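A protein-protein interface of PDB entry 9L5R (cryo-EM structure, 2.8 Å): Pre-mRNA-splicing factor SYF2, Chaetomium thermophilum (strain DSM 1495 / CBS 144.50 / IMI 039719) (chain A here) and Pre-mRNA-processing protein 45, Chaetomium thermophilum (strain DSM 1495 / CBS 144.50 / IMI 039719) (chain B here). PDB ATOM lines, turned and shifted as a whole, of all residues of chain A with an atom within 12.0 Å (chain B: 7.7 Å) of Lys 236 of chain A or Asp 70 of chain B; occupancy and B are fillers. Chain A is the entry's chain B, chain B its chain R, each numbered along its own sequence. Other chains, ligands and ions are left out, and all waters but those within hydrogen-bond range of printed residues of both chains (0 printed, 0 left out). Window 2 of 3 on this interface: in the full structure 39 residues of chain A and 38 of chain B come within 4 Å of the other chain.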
ATOM      1  N   ALA A 211     -35.861   3.332   8.761  1.00  0.00           N
ATOM      2  CA  ALA A 211     -34.441   3.634   8.696  1.00  0.00           C
ATOM      3  C   ALA A 211     -34.163   5.079   9.069  1.00  0.00           C
ATOM      4  O   ALA A 211     -33.111   5.368   9.640  1.00  0.00           O
ATOM      5  CB  ALA A 211     -33.901   3.331   7.302  1.00  0.00           C
ATOM      6  N   ILE A 212     -35.098   5.988   8.782  1.00  0.00           N
ATOM      7  CA  ILE A 212     -34.918   7.389   9.152  1.00  0.00           C
ATOM      8  C   ILE A 212     -34.883   7.538  10.665  1.00  0.00           C
ATOM      9  O   ILE A 212     -33.972   8.159  11.218  1.00  0.00           O
ATOM     10  CB  ILE A 212     -36.017   8.266   8.529  1.00  0.00           C
ATOM     11  CG1 ILE A 212     -35.688   8.605   7.083  1.00  0.00           C
ATOM     12  CG2 ILE A 212     -36.172   9.566   9.294  1.00  0.00           C
ATOM     13  CD1 ILE A 212     -36.905   8.976   6.286  1.00  0.00           C
ATOM     14  N   LYS A 214     -34.369   5.143  12.910  1.00  0.00           N
ATOM     15  CA  LYS A 214     -33.261   4.378  13.476  1.00  0.00           C
ATOM     16  C   LYS A 214     -31.927   5.095  13.291  1.00  0.00           C
ATOM     17  O   LYS A 214     -31.122   5.165  14.227  1.00  0.00           O
ATOM     18  CB  LYS A 214     -33.216   2.983  12.853  1.00  0.00           C
ATOM     19  CG  LYS A 214     -31.890   2.268  13.037  1.00  0.00           C
ATOM     20  CD  LYS A 214     -32.028   0.765  12.912  1.00  0.00           C
ATOM     21  CE  LYS A 214     -30.788   0.171  12.263  1.00  0.00           C
ATOM     22  NZ  LYS A 214     -30.774  -1.316  12.289  1.00  0.00           N
ATOM     23  N   ALA A 215     -31.677   5.652  12.105  1.00  0.00           N
ATOM     24  CA  ALA A 215     -30.437   6.381  11.878  1.00  0.00           C
ATOM     25  C   ALA A 215     -30.418   7.704  12.624  1.00  0.00           C
ATOM     26  O   ALA A 215     -29.344   8.183  12.998  1.00  0.00           O
ATOM     27  CB  ALA A 215     -30.236   6.613  10.384  1.00  0.00           C
ATOM     28  N   ALA A 216     -31.587   8.307  12.847  1.00  0.00           N
ATOM     29  CA  ALA A 216     -31.655   9.488  13.695  1.00  0.00           C
ATOM     30  C   ALA A 216     -31.278   9.148  15.126  1.00  0.00           C
ATOM     31  O   ALA A 216     -30.544   9.900  15.771  1.00  0.00           O
ATOM     32  CB  ALA A 216     -33.052  10.100  13.637  1.00  0.00           C
ATOM     33  N   ALA A 217     -31.760   8.009  15.632  1.00  0.00           N
ATOM     34  CA  ALA A 217     -31.375   7.562  16.967  1.00  0.00           C
ATOM     35  C   ALA A 217     -29.890   7.231  17.039  1.00  0.00           C
ATOM     36  O   ALA A 217     -29.231   7.522  18.041  1.00  0.00           O
ATOM     37  CB  ALA A 217     -32.213   6.353  17.378  1.00  0.00           C
ATOM     38  N   ALA A 218     -29.347   6.626  15.987  1.00  0.00           N
ATOM     39  CA  ALA A 218     -27.937   6.266  15.941  1.00  0.00           C
ATOM     40  C   ALA A 218     -27.030   7.442  15.613  1.00  0.00           C
ATOM     41  O   ALA A 218     -25.808   7.274  15.614  1.00  0.00           O
ATOM     42  CB  ALA A 218     -27.710   5.151  14.919  1.00  0.00           C
ATOM     43  N   GLY A 219     -27.587   8.607  15.308  1.00  0.00           N
ATOM     44  CA  GLY A 219     -26.791   9.800  15.151  1.00  0.00           C
ATOM     45  C   GLY A 219     -26.189  10.011  13.783  1.00  0.00           C
ATOM     46  O   GLY A 219     -25.419  10.963  13.607  1.00  0.00           O
ATOM     47  N   THR A 220     -26.501   9.159  12.812  1.00  0.00           N
ATOM     48  CA  THR A 220     -26.033   9.358  11.449  1.00  0.00           C
ATOM     49  C   THR A 220     -26.993  10.185  10.607  1.00  0.00           C
ATOM     50  O   THR A 220     -26.656  10.524   9.472  1.00  0.00           O
ATOM     51  CB  THR A 220     -25.792   8.010  10.764  1.00  0.00           C
ATOM     52  OG1 THR A 220     -27.047   7.395  10.461  1.00  0.00           O
ATOM     53  CG2 THR A 220     -24.997   7.091  11.665  1.00  0.00           C
ATOM     54  N   LEU A 221     -28.171  10.512  11.127  1.00  0.00           N
ATOM     55  CA  LEU A 221     -29.128  11.372  10.444  1.00  0.00           C
ATOM     56  C   LEU A 221     -29.446  12.559  11.337  1.00  0.00           C
ATOM     57  O   LEU A 221     -29.766  12.382  12.516  1.00  0.00           O
ATOM     58  CB  LEU A 221     -30.419  10.624  10.104  1.00  0.00           C
ATOM     59  CG  LEU A 221     -30.598  10.038   8.703  1.00  0.00           C
ATOM     60  CD1 LEU A 221     -31.926   9.365   8.606  1.00  0.00           C
ATOM     61  CD2 LEU A 221     -30.516  11.098   7.652  1.00  0.00           C
ATOM     62  N   ASP A 222     -29.356  13.759  10.776  1.00  0.00           N
ATOM     63  CA  ASP A 222     -29.746  14.984  11.461  1.00  0.00           C
ATOM     64  C   ASP A 222     -31.089  15.439  10.917  1.00  0.00           C
ATOM     65  O   ASP A 222     -31.220  15.665   9.714  1.00  0.00           O
ATOM     66  CB  ASP A 222     -28.708  16.087  11.269  1.00  0.00           C
ATOM     67  CG  ASP A 222     -27.603  16.034  12.294  1.00  0.00           C
ATOM     68  OD1 ASP A 222     -27.796  15.395  13.348  1.00  0.00           O
ATOM     69  OD2 ASP A 222     -26.547  16.654  12.057  1.00  0.00           O
ATOM     70  N   ILE A 223     -32.076  15.575  11.793  1.00  0.00           N
ATOM     71  CA  ILE A 223     -33.362  16.148  11.416  1.00  0.00           C
ATOM     72  C   ILE A 223     -33.275  17.650  11.643  1.00  0.00           C
ATOM     73  O   ILE A 223     -33.157  18.108  12.781  1.00  0.00           O
ATOM     74  CB  ILE A 223     -34.515  15.533  12.212  1.00  0.00           C
ATOM     75  CG1 ILE A 223     -34.573  14.022  11.986  1.00  0.00           C
ATOM     76  CG2 ILE A 223     -35.821  16.199  11.827  1.00  0.00           C
ATOM     77  CD1 ILE A 223     -35.827  13.362  12.535  1.00  0.00           C
ATOM     78  N   ILE A 224     -33.330  18.422  10.561  1.00  0.00           N
ATOM     79  CA  ILE A 224     -33.190  19.865  10.635  1.00  0.00           C
ATOM     80  C   ILE A 224     -34.425  20.518  10.032  1.00  0.00           C
ATOM     81  O   ILE A 224     -35.194  19.903   9.284  1.00  0.00           O
ATOM     82  CB  ILE A 224     -31.917  20.369   9.925  1.00  0.00           C
ATOM     83  CG1 ILE A 224     -31.986  20.065   8.429  1.00  0.00           C
ATOM     84  CG2 ILE A 224     -30.673  19.758  10.548  1.00  0.00           C
ATOM     85  CD1 ILE A 224     -30.859  20.667   7.633  1.00  0.00           C
ATOM     86  N   ILE A 232     -36.130  18.128   7.129  1.00  0.00           N
ATOM     87  CA  ILE A 232     -35.094  17.720   6.190  1.00  0.00           C
ATOM     88  C   ILE A 232     -34.131  16.815   6.937  1.00  0.00           C
ATOM     89  O   ILE A 232     -33.565  17.213   7.961  1.00  0.00           O
ATOM     90  CB  ILE A 232     -34.359  18.922   5.582  1.00  0.00           C
ATOM     91  CG1 ILE A 232     -35.319  19.771   4.759  1.00  0.00           C
ATOM     92  CG2 ILE A 232     -33.212  18.456   4.717  1.00  0.00           C
ATOM     93  CD1 ILE A 232     -36.029  19.002   3.672  1.00  0.00           C
ATOM     94  N   ALA A 233     -33.948  15.603   6.438  1.00  0.00           N
ATOM     95  CA  ALA A 233     -32.984  14.689   7.021  1.00  0.00           C
ATOM     96  C   ALA A 233     -31.656  14.830   6.300  1.00  0.00           C
ATOM     97  O   ALA A 233     -31.612  14.968   5.077  1.00  0.00           O
ATOM     98  CB  ALA A 233     -33.484  13.249   6.937  1.00  0.00           C
ATOM     99  N   VAL A 234     -30.571  14.823   7.065  1.00  0.00           N
ATOM    100  CA  VAL A 234     -29.230  14.933   6.512  1.00  0.00           C
ATOM    101  C   VAL A 234     -28.431  13.711   6.925  1.00  0.00           C
ATOM    102  O   VAL A 234     -28.230  13.470   8.121  1.00  0.00           O
ATOM    103  CB  VAL A 234     -28.510  16.206   6.962  1.00  0.00           C
ATOM    104  CG1 VAL A 234     -27.117  16.183   6.393  1.00  0.00           C
ATOM    105  CG2 VAL A 234     -29.260  17.429   6.491  1.00  0.00           C
ATOM    106  N   ASP A 235     -27.978  12.945   5.938  1.00  0.00           N
ATOM    107  CA  ASP A 235     -27.088  11.818   6.174  1.00  0.00           C
ATOM    108  C   ASP A 235     -25.688  12.364   6.413  1.00  0.00           C
ATOM    109  O   ASP A 235     -25.089  12.964   5.516  1.00  0.00           O
ATOM    110  CB  ASP A 235     -27.120  10.866   4.985  1.00  0.00           C
ATOM    111  CG  ASP A 235     -26.793   9.442   5.370  1.00  0.00           C
ATOM    112  OD1 ASP A 235     -27.061   9.055   6.524  1.00  0.00           O
ATOM    113  OD2 ASP A 235     -26.270   8.704   4.512  1.00  0.00           O
ATOM    114  N   LYS A 236     -25.178  12.183   7.633  1.00  0.00           N
ATOM    115  CA  LYS A 236     -23.857  12.693   7.980  1.00  0.00           C
ATOM    116  C   LYS A 236     -22.772  11.956   7.207  1.00  0.00           C
ATOM    117  O   LYS A 236     -21.864  12.573   6.638  1.00  0.00           O
ATOM    118  CB  LYS A 236     -23.643  12.561   9.485  1.00  0.00           C
ATOM    119  CG  LYS A 236     -24.738  13.206  10.314  1.00  0.00           C
ATOM    120  CD  LYS A 236     -24.834  14.691  10.040  1.00  0.00           C
ATOM    121  CE  LYS A 236     -23.609  15.425  10.559  1.00  0.00           C
ATOM    122  NZ  LYS A 236     -23.489  15.319  12.039  1.00  0.00           N
ATOM    123  N   ASP A 237     -22.852  10.632   7.180  1.00  0.00           N
ATOM    124  CA  ASP A 237     -22.117   9.806   6.238  1.00  0.00           C
ATOM    125  C   ASP A 237     -22.946   9.676   4.960  1.00  0.00           C
ATOM    126  O   ASP A 237     -23.887  10.436   4.732  1.00  0.00           O
ATOM    127  CB  ASP A 237     -21.764   8.469   6.886  1.00  0.00           C
ATOM    128  CG  ASP A 237     -22.973   7.756   7.459  1.00  0.00           C
ATOM    129  OD1 ASP A 237     -24.083   8.323   7.428  1.00  0.00           O
ATOM    130  OD2 ASP A 237     -22.813   6.625   7.955  1.00  0.00           O
ATOM    131  N   GLY A 238     -22.591   8.745   4.088  1.00  0.00           N
ATOM    132  CA  GLY A 238     -23.402   8.536   2.907  1.00  0.00           C
ATOM    133  C   GLY A 238     -24.034   7.164   2.875  1.00  0.00           C
ATOM    134  O   GLY A 238     -24.361   6.646   1.804  1.00  0.00           O
ATOM    135  N   THR A 239     -24.224   6.569   4.046  1.00  0.00           N
ATOM    136  CA  THR A 239     -24.571   5.161   4.153  1.00  0.00           C
ATOM    137  C   THR A 239     -26.051   4.917   4.399  1.00  0.00           C
ATOM    138  O   THR A 239     -26.429   3.778   4.686  1.00  0.00           O
ATOM    139  CB  THR A 239     -23.753   4.500   5.262  1.00  0.00           C
ATOM    140  OG1 THR A 239     -24.232   4.945   6.534  1.00  0.00           O
ATOM    141  CG2 THR A 239     -22.294   4.866   5.127  1.00  0.00           C
ATOM    142  N   PHE A 240     -26.895   5.950   4.317  1.00  0.00           N
ATOM    143  CA  PHE A 240     -28.330   5.715   4.422  1.00  0.00           C
ATOM    144  C   PHE A 240     -28.836   4.890   3.251  1.00  0.00           C
ATOM    145  O   PHE A 240     -29.481   3.853   3.437  1.00  0.00           O
ATOM    146  CB  PHE A 240     -29.099   7.035   4.497  1.00  0.00           C
ATOM    147  CG  PHE A 240     -30.561   6.855   4.748  1.00  0.00           C
ATOM    148  CD1 PHE A 240     -31.026   6.612   6.024  1.00  0.00           C
ATOM    149  CD2 PHE A 240     -31.468   6.890   3.709  1.00  0.00           C
ATOM    150  CE1 PHE A 240     -32.364   6.424   6.256  1.00  0.00           C
ATOM    151  CE2 PHE A 240     -32.804   6.688   3.935  1.00  0.00           C
ATOM    152  CZ  PHE A 240     -33.254   6.464   5.210  1.00  0.00           C
ATOM    153  N   PHE A 241     -28.538   5.325   2.037  1.00  0.00           N
ATOM    154  CA  PHE A 241     -29.151   4.726   0.866  1.00  0.00           C
ATOM    155  C   PHE A 241     -28.425   3.488   0.384  1.00  0.00           C
ATOM    156  O   PHE A 241     -29.047   2.630  -0.237  1.00  0.00           O
ATOM    157  CB  PHE A 241     -29.228   5.749  -0.262  1.00  0.00           C
ATOM    158  CG  PHE A 241     -30.340   6.726  -0.101  1.00  0.00           C
ATOM    159  CD1 PHE A 241     -31.650   6.304  -0.133  1.00  0.00           C
ATOM    160  CD2 PHE A 241     -30.076   8.064   0.094  1.00  0.00           C
ATOM    161  CE1 PHE A 241     -32.678   7.198   0.014  1.00  0.00           C
ATOM    162  CE2 PHE A 241     -31.098   8.964   0.246  1.00  0.00           C
ATOM    163  CZ  PHE A 241     -32.402   8.531   0.205  1.00  0.00           C
ATOM    164  N   SER A 242     -27.136   3.367   0.659  1.00  0.00           N
ATOM    165  CA  SER A 242     -26.342   2.252   0.175  1.00  0.00           C
ATOM    166  C   SER A 242     -25.512   1.682   1.311  1.00  0.00           C
ATOM    167  O   SER A 242     -24.993   2.428   2.142  1.00  0.00           O
ATOM    168  CB  SER A 242     -25.433   2.691  -0.974  1.00  0.00           C
ATOM    169  OG  SER A 242     -24.493   1.691  -1.289  1.00  0.00           O
ATOM    170  N   ALA A 244     -22.735   0.194   0.728  1.00  0.00           N
ATOM    171  CA  ALA A 244     -21.352   0.527   0.439  1.00  0.00           C
ATOM    172  C   ALA A 244     -20.946   1.697   1.317  1.00  0.00           C
ATOM    173  O   ALA A 244     -21.738   2.622   1.535  1.00  0.00           O
ATOM    174  CB  ALA A 244     -21.172   0.875  -1.034  1.00  0.00           C
ATOM    175  N   ASN A 245     -19.722   1.628   1.845  1.00  0.00           N
ATOM    176  CA  ASN A 245     -19.149   2.467   2.900  1.00  0.00           C
ATOM    177  C   ASN A 245     -19.780   2.246   4.269  1.00  0.00           C
ATOM    178  O   ASN A 245     -19.368   2.899   5.226  1.00  0.00           O
ATOM    179  CB  ASN A 245     -19.201   3.969   2.580  1.00  0.00           C
ATOM    180  CG  ASN A 245     -17.999   4.695   3.069  1.00  0.00           C
ATOM    181  OD1 ASN A 245     -16.930   4.119   3.186  1.00  0.00           O
ATOM    182  ND2 ASN A 245     -18.159   5.971   3.365  1.00  0.00           N
ATOM    183  N   ALA A 246     -20.752   1.354   4.402  1.00  0.00           N
ATOM    184  CA  ALA A 246     -21.311   1.024   5.703  1.00  0.00           C
ATOM    185  C   ALA A 246     -20.511  -0.116   6.311  1.00  0.00           C
ATOM    186  O   ALA A 246     -20.327  -1.156   5.674  1.00  0.00           O
ATOM    187  CB  ALA A 246     -22.782   0.634   5.581  1.00  0.00           C
ATOM    188  N   ILE B  33     -34.073  13.468   2.049  1.00  0.00           N
ATOM    189  CA  ILE B  33     -32.854  13.071   2.733  1.00  0.00           C
ATOM    190  C   ILE B  33     -31.714  13.512   1.835  1.00  0.00           C
ATOM    191  O   ILE B  33     -31.575  13.027   0.707  1.00  0.00           O
ATOM    192  CB  ILE B  33     -32.808  11.569   3.012  1.00  0.00           C
ATOM    193  CG1 ILE B  33     -33.982  11.190   3.900  1.00  0.00           C
ATOM    194  CG2 ILE B  33     -31.502  11.192   3.676  1.00  0.00           C
ATOM    195  CD1 ILE B  33     -34.419   9.800   3.731  1.00  0.00           C
ATOM    196  N   VAL B  34     -30.905  14.446   2.319  1.00  0.00           N
ATOM    197  CA  VAL B  34     -29.881  15.058   1.488  1.00  0.00           C
ATOM    198  C   VAL B  34     -28.641  15.144   2.375  1.00  0.00           C
ATOM    199  O   VAL B  34     -28.610  14.517   3.434  1.00  0.00           O
ATOM    200  CB  VAL B  34     -30.374  16.408   0.934  1.00  0.00           C
ATOM    201  CG1 VAL B  34     -30.578  17.445   2.038  1.00  0.00           C
ATOM    202  CG2 VAL B  34     -29.605  16.852  -0.318  1.00  0.00           C
ATOM    203  N   SER B  35     -27.587  15.829   1.945  1.00  0.00           N
ATOM    204  CA  SER B  35     -26.311  15.747   2.645  1.00  0.00           C
ATOM    205  C   SER B  35     -25.801  17.120   3.111  1.00  0.00           C
ATOM    206  O   SER B  35     -26.481  18.157   3.013  1.00  0.00           O
ATOM    207  CB  SER B  35     -25.280  15.056   1.753  1.00  0.00           C
ATOM    208  OG  SER B  35     -25.050  15.812   0.580  1.00  0.00           O
ATOM    209  N   ALA B  36     -24.569  17.105   3.632  1.00  0.00           N
ATOM    210  CA  ALA B  36     -23.921  18.316   4.123  1.00  0.00           C
ATOM    211  C   ALA B  36     -23.639  19.311   3.008  1.00  0.00           C
ATOM    212  O   ALA B  36     -23.486  20.505   3.286  1.00  0.00           O
ATOM    213  CB  ALA B  36     -22.624  17.959   4.845  1.00  0.00           C
ATOM    214  N   ILE B  39     -26.656  21.172   3.269  1.00  0.00           N
ATOM    215  CA  ILE B  39     -26.523  22.032   4.449  1.00  0.00           C
ATOM    216  C   ILE B  39     -25.777  23.312   4.090  1.00  0.00           C
ATOM    217  O   ILE B  39     -26.219  24.423   4.411  1.00  0.00           O
ATOM    218  CB  ILE B  39     -25.812  21.303   5.605  1.00  0.00           C
ATOM    219  CG1 ILE B  39     -26.657  20.178   6.187  1.00  0.00           C
ATOM    220  CG2 ILE B  39     -25.417  22.284   6.709  1.00  0.00           C
ATOM    221  CD1 ILE B  39     -25.902  19.427   7.259  1.00  0.00           C
ATOM    222  N   PRO B  65     -26.462   8.179  20.755  1.00  0.00           N
ATOM    223  CA  PRO B  65     -25.565   8.991  19.919  1.00  0.00           C
ATOM    224  C   PRO B  65     -26.172  10.305  19.444  1.00  0.00           C
ATOM    225  O   PRO B  65     -25.411  11.198  19.045  1.00  0.00           O
ATOM    226  CB  PRO B  65     -25.244   8.054  18.752  1.00  0.00           C
ATOM    227  CG  PRO B  65     -25.336   6.698  19.346  1.00  0.00           C
ATOM    228  CD  PRO B  65     -26.444   6.761  20.350  1.00  0.00           C
ATOM    229  N   GLU B  66     -27.504  10.447  19.462  1.00  0.00           N
ATOM    230  CA  GLU B  66     -28.117  11.771  19.401  1.00  0.00           C
ATOM    231  C   GLU B  66     -27.523  12.679  20.464  1.00  0.00           C
ATOM    232  O   GLU B  66     -27.092  13.802  20.180  1.00  0.00           O
ATOM    233  CB  GLU B  66     -29.624  11.684  19.639  1.00  0.00           C
ATOM    234  CG  GLU B  66     -30.395  10.697  18.826  1.00  0.00           C
ATOM    235  CD  GLU B  66     -31.820  10.549  19.331  1.00  0.00           C
ATOM    236  OE1 GLU B  66     -32.066  10.882  20.509  1.00  0.00           O
ATOM    237  OE2 GLU B  66     -32.697  10.122  18.554  1.00  0.00           O
ATOM    238  N   ASP B  67     -27.494  12.191  21.704  1.00  0.00           N
ATOM    239  CA  ASP B  67     -27.022  12.992  22.822  1.00  0.00           C
ATOM    240  C   ASP B  67     -25.518  13.192  22.766  1.00  0.00           C
ATOM    241  O   ASP B  67     -25.013  14.211  23.244  1.00  0.00           O
ATOM    242  CB  ASP B  67     -27.435  12.331  24.130  1.00  0.00           C
ATOM    243  CG  ASP B  67     -28.918  12.063  24.190  1.00  0.00           C
ATOM    244  OD1 ASP B  67     -29.683  12.819  23.556  1.00  0.00           O
ATOM    245  OD2 ASP B  67     -29.324  11.100  24.864  1.00  0.00           O
ATOM    246  N   PHE B  68     -24.788  12.240  22.191  1.00  0.00           N
ATOM    247  CA  PHE B  68     -23.370  12.494  21.957  1.00  0.00           C
ATOM    248  C   PHE B  68     -23.140  13.496  20.833  1.00  0.00           C
ATOM    249  O   PHE B  68     -22.078  14.123  20.788  1.00  0.00           O
ATOM    250  CB  PHE B  68     -22.640  11.187  21.663  1.00  0.00           C
ATOM    251  CG  PHE B  68     -22.679  10.228  22.801  1.00  0.00           C
ATOM    252  CD1 PHE B  68     -21.925  10.454  23.929  1.00  0.00           C
ATOM    253  CD2 PHE B  68     -23.490   9.118  22.757  1.00  0.00           C
ATOM    254  CE1 PHE B  68     -21.975   9.587  24.978  1.00  0.00           C
ATOM    255  CE2 PHE B  68     -23.547   8.246  23.806  1.00  0.00           C
ATOM    256  CZ  PHE B  68     -22.793   8.479  24.916  1.00  0.00           C
ATOM    257  N   GLY B  69     -24.108  13.664  19.935  1.00  0.00           N
ATOM    258  CA  GLY B  69     -23.967  14.601  18.840  1.00  0.00           C
ATOM    259  C   GLY B  69     -23.137  14.009  17.724  1.00  0.00           C
ATOM    260  O   GLY B  69     -23.508  12.986  17.143  1.00  0.00           O
ATOM    261  N   ASP B  70     -22.001  14.634  17.423  1.00  0.00           N
ATOM    262  CA  ASP B  70     -20.984  14.020  16.582  1.00  0.00           C
ATOM    263  C   ASP B  70     -19.986  13.214  17.396  1.00  0.00           C
ATOM    264  O   ASP B  70     -18.808  13.124  17.027  1.00  0.00           O
ATOM    265  CB  ASP B  70     -20.276  15.076  15.737  1.00  0.00           C
ATOM    266  CG  ASP B  70     -21.167  15.643  14.653  1.00  0.00           C
ATOM    267  OD1 ASP B  70     -22.053  14.903  14.179  1.00  0.00           O
ATOM    268  OD2 ASP B  70     -20.988  16.822  14.276  1.00  0.00           O
ATOM    269  N   GLY B  71     -20.427  12.673  18.528  1.00  0.00           N
ATOM    270  CA  GLY B  71     -19.692  11.665  19.254  1.00  0.00           C
ATOM    271  C   GLY B  71     -18.704  12.240  20.240  1.00  0.00           C
ATOM    272  O   GLY B  71     -18.474  13.446  20.320  1.00  0.00           O
ATOM    273  N   GLY B  72     -18.107  11.334  21.006  1.00  0.00           N
ATOM    274  CA  GLY B  72     -17.204  11.705  22.068  1.00  0.00           C
ATOM    275  C   GLY B  72     -17.819  11.478  23.426  1.00  0.00           C
ATOM    276  O   GLY B  72     -18.790  12.144  23.790  1.00  0.00           O
ATOM    277  N   PRO B  83     -20.454   6.228  22.150  1.00  0.00           N
ATOM    278  CA  PRO B  83     -20.828   7.239  21.146  1.00  0.00           C
ATOM    279  C   PRO B  83     -21.338   6.675  19.829  1.00  0.00           C
ATOM    280  O   PRO B  83     -22.005   7.400  19.086  1.00  0.00           O
ATOM    281  CB  PRO B  83     -19.526   8.021  20.944  1.00  0.00           C
ATOM    282  CG  PRO B  83     -18.780   7.828  22.194  1.00  0.00           C
ATOM    283  CD  PRO B  83     -19.095   6.446  22.660  1.00  0.00           C
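Among the printed residues, merely in contact across the chains: Ala 216 of chain A with Glu 66 of chain B, Val 234 of chain A with Val 34 of chain B, Ala 233 of chain A with Ile 33 of chain B, Ala 218 of chain A with Pro 65 of chain B, Ala 217 of chain A with Glu 66 of chain B, Phe 240 of chain A with Ile 33 of chain B, Val 234 of chain A with Ile 39 of chain B, Val 234 of chain A with Ser 35 of chain B, Ile 212 of chain A with Ile 33 of chain B, Ala 217 of chain A with Pro 65 of chain B, Val 234 of chain A with Ala 36 of chain B and Ile 232 of chain A with Val 34 of chain B.
Lys 236 of chain A touches just one residue of chain B: Asp 70 (2.6 Å).
Printed residues of chain A within 4 Å of Asp 70 of chain B: Lys 236.
Of chain A, only Val 234 (3.7 Å) comes within 4 Å of Ser 35 of chain B.
No residue of chain A comes within 4 Å of Gly 69 of chain B.
Gly 71 of chain B touches none of the printed residues of chain A.
No residue of chain A comes within 4 Å of Gly 72 of chain B.
Of the printed residues of chain A, Glu 66 of chain B touches Ala 216 (3.2 Å) and Ala 217 (3.3 Å).
Of the printed residues of chain A, Pro 65 of chain B touches Ala 217 (3.7 Å) and Ala 218 (3.3 Å).
Of the printed residues of chain A, Ile 39 of chain B touches Val 234 (3.6 Å).
Ser 242 of chain A touches none of the printed residues of chain B.
Lys 214 of chain A touches none of the printed residues of chain B.
The nearest residue of chain A that does not touch Asp 70 of chain B is Gly 219 of chain A (5.2 Å).
NZ of Lys 236 of chain A lies within salt-bridge range of OD1 of Asp 70 of chain B.
The backbone carbonyl oxygen (O) of Val 34 of chain B lies within hydrogen-bond range of the backbone NH (N) of Asp 235 of chain A (3.0 Å).
The backbone carbonyl oxygen (O) of Ala 233 of chain A sits at hydrogen-bond distance from the backbone NH (N) of Val 34 of chain B (2.9 Å).
Of the 27 printed residues of chain A, 10 touch a printed residue of chain B.
Hydrophobic or aromatic side chains of chain A that line the printed part of chain B: Ile 212, Ala 217, Ile 232, Ala 233, Val 234 and Phe 240.
Of the 14 printed residues of chain B, 8 touch a printed residue of chain A.
Printed residues of chain B that touch a printed residue of chain A: Ile 33, Val 34, Ser 35, Ala 36, Ile 39, Pro 65, Glu 66 and Asp 70.
Hydrophobic or aromatic side chains of chain B that line the printed part of chain A: Ile 33, Val 34, Ile 39 and Pro 65.
Among the printed residues, Asp or Glu carboxylates within 4 Å of a Lys or Arg side-chain nitrogen of the other chain: Lys 236 of chain A with Asp 70 of chain B (2.6 Å).
The backbone NH (N) of Lys 236 of chain A sits at hydrogen-bond distance from the backbone carbonyl oxygen (O) of Thr 220 of chain A.
The side-chain carboxylate (OD2) of Asp 235 of chain A is in hydrogen-bond range of the backbone NH (N) of Thr 239 of chain A.
O of Asp 222 of chain A is in hydrogen-bond range of N of Val 234 of chain A.
The side-chain carboxylate (OD2) of Asp 235 of chain A is in hydrogen-bond range of the backbone NH (N) of Phe 240 of chain A, 2.8 Å away.
The backbone NH (N) of Ile 224 of chain A sits at hydrogen-bond distance from the backbone carbonyl oxygen (O) of Ile 232 of chain A (2.9 Å).
The side-chain amino group of Lys 236 of chain A lies within salt-bridge range of the side-chain carboxylate of Asp 222 of chain A (3.3 Å).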
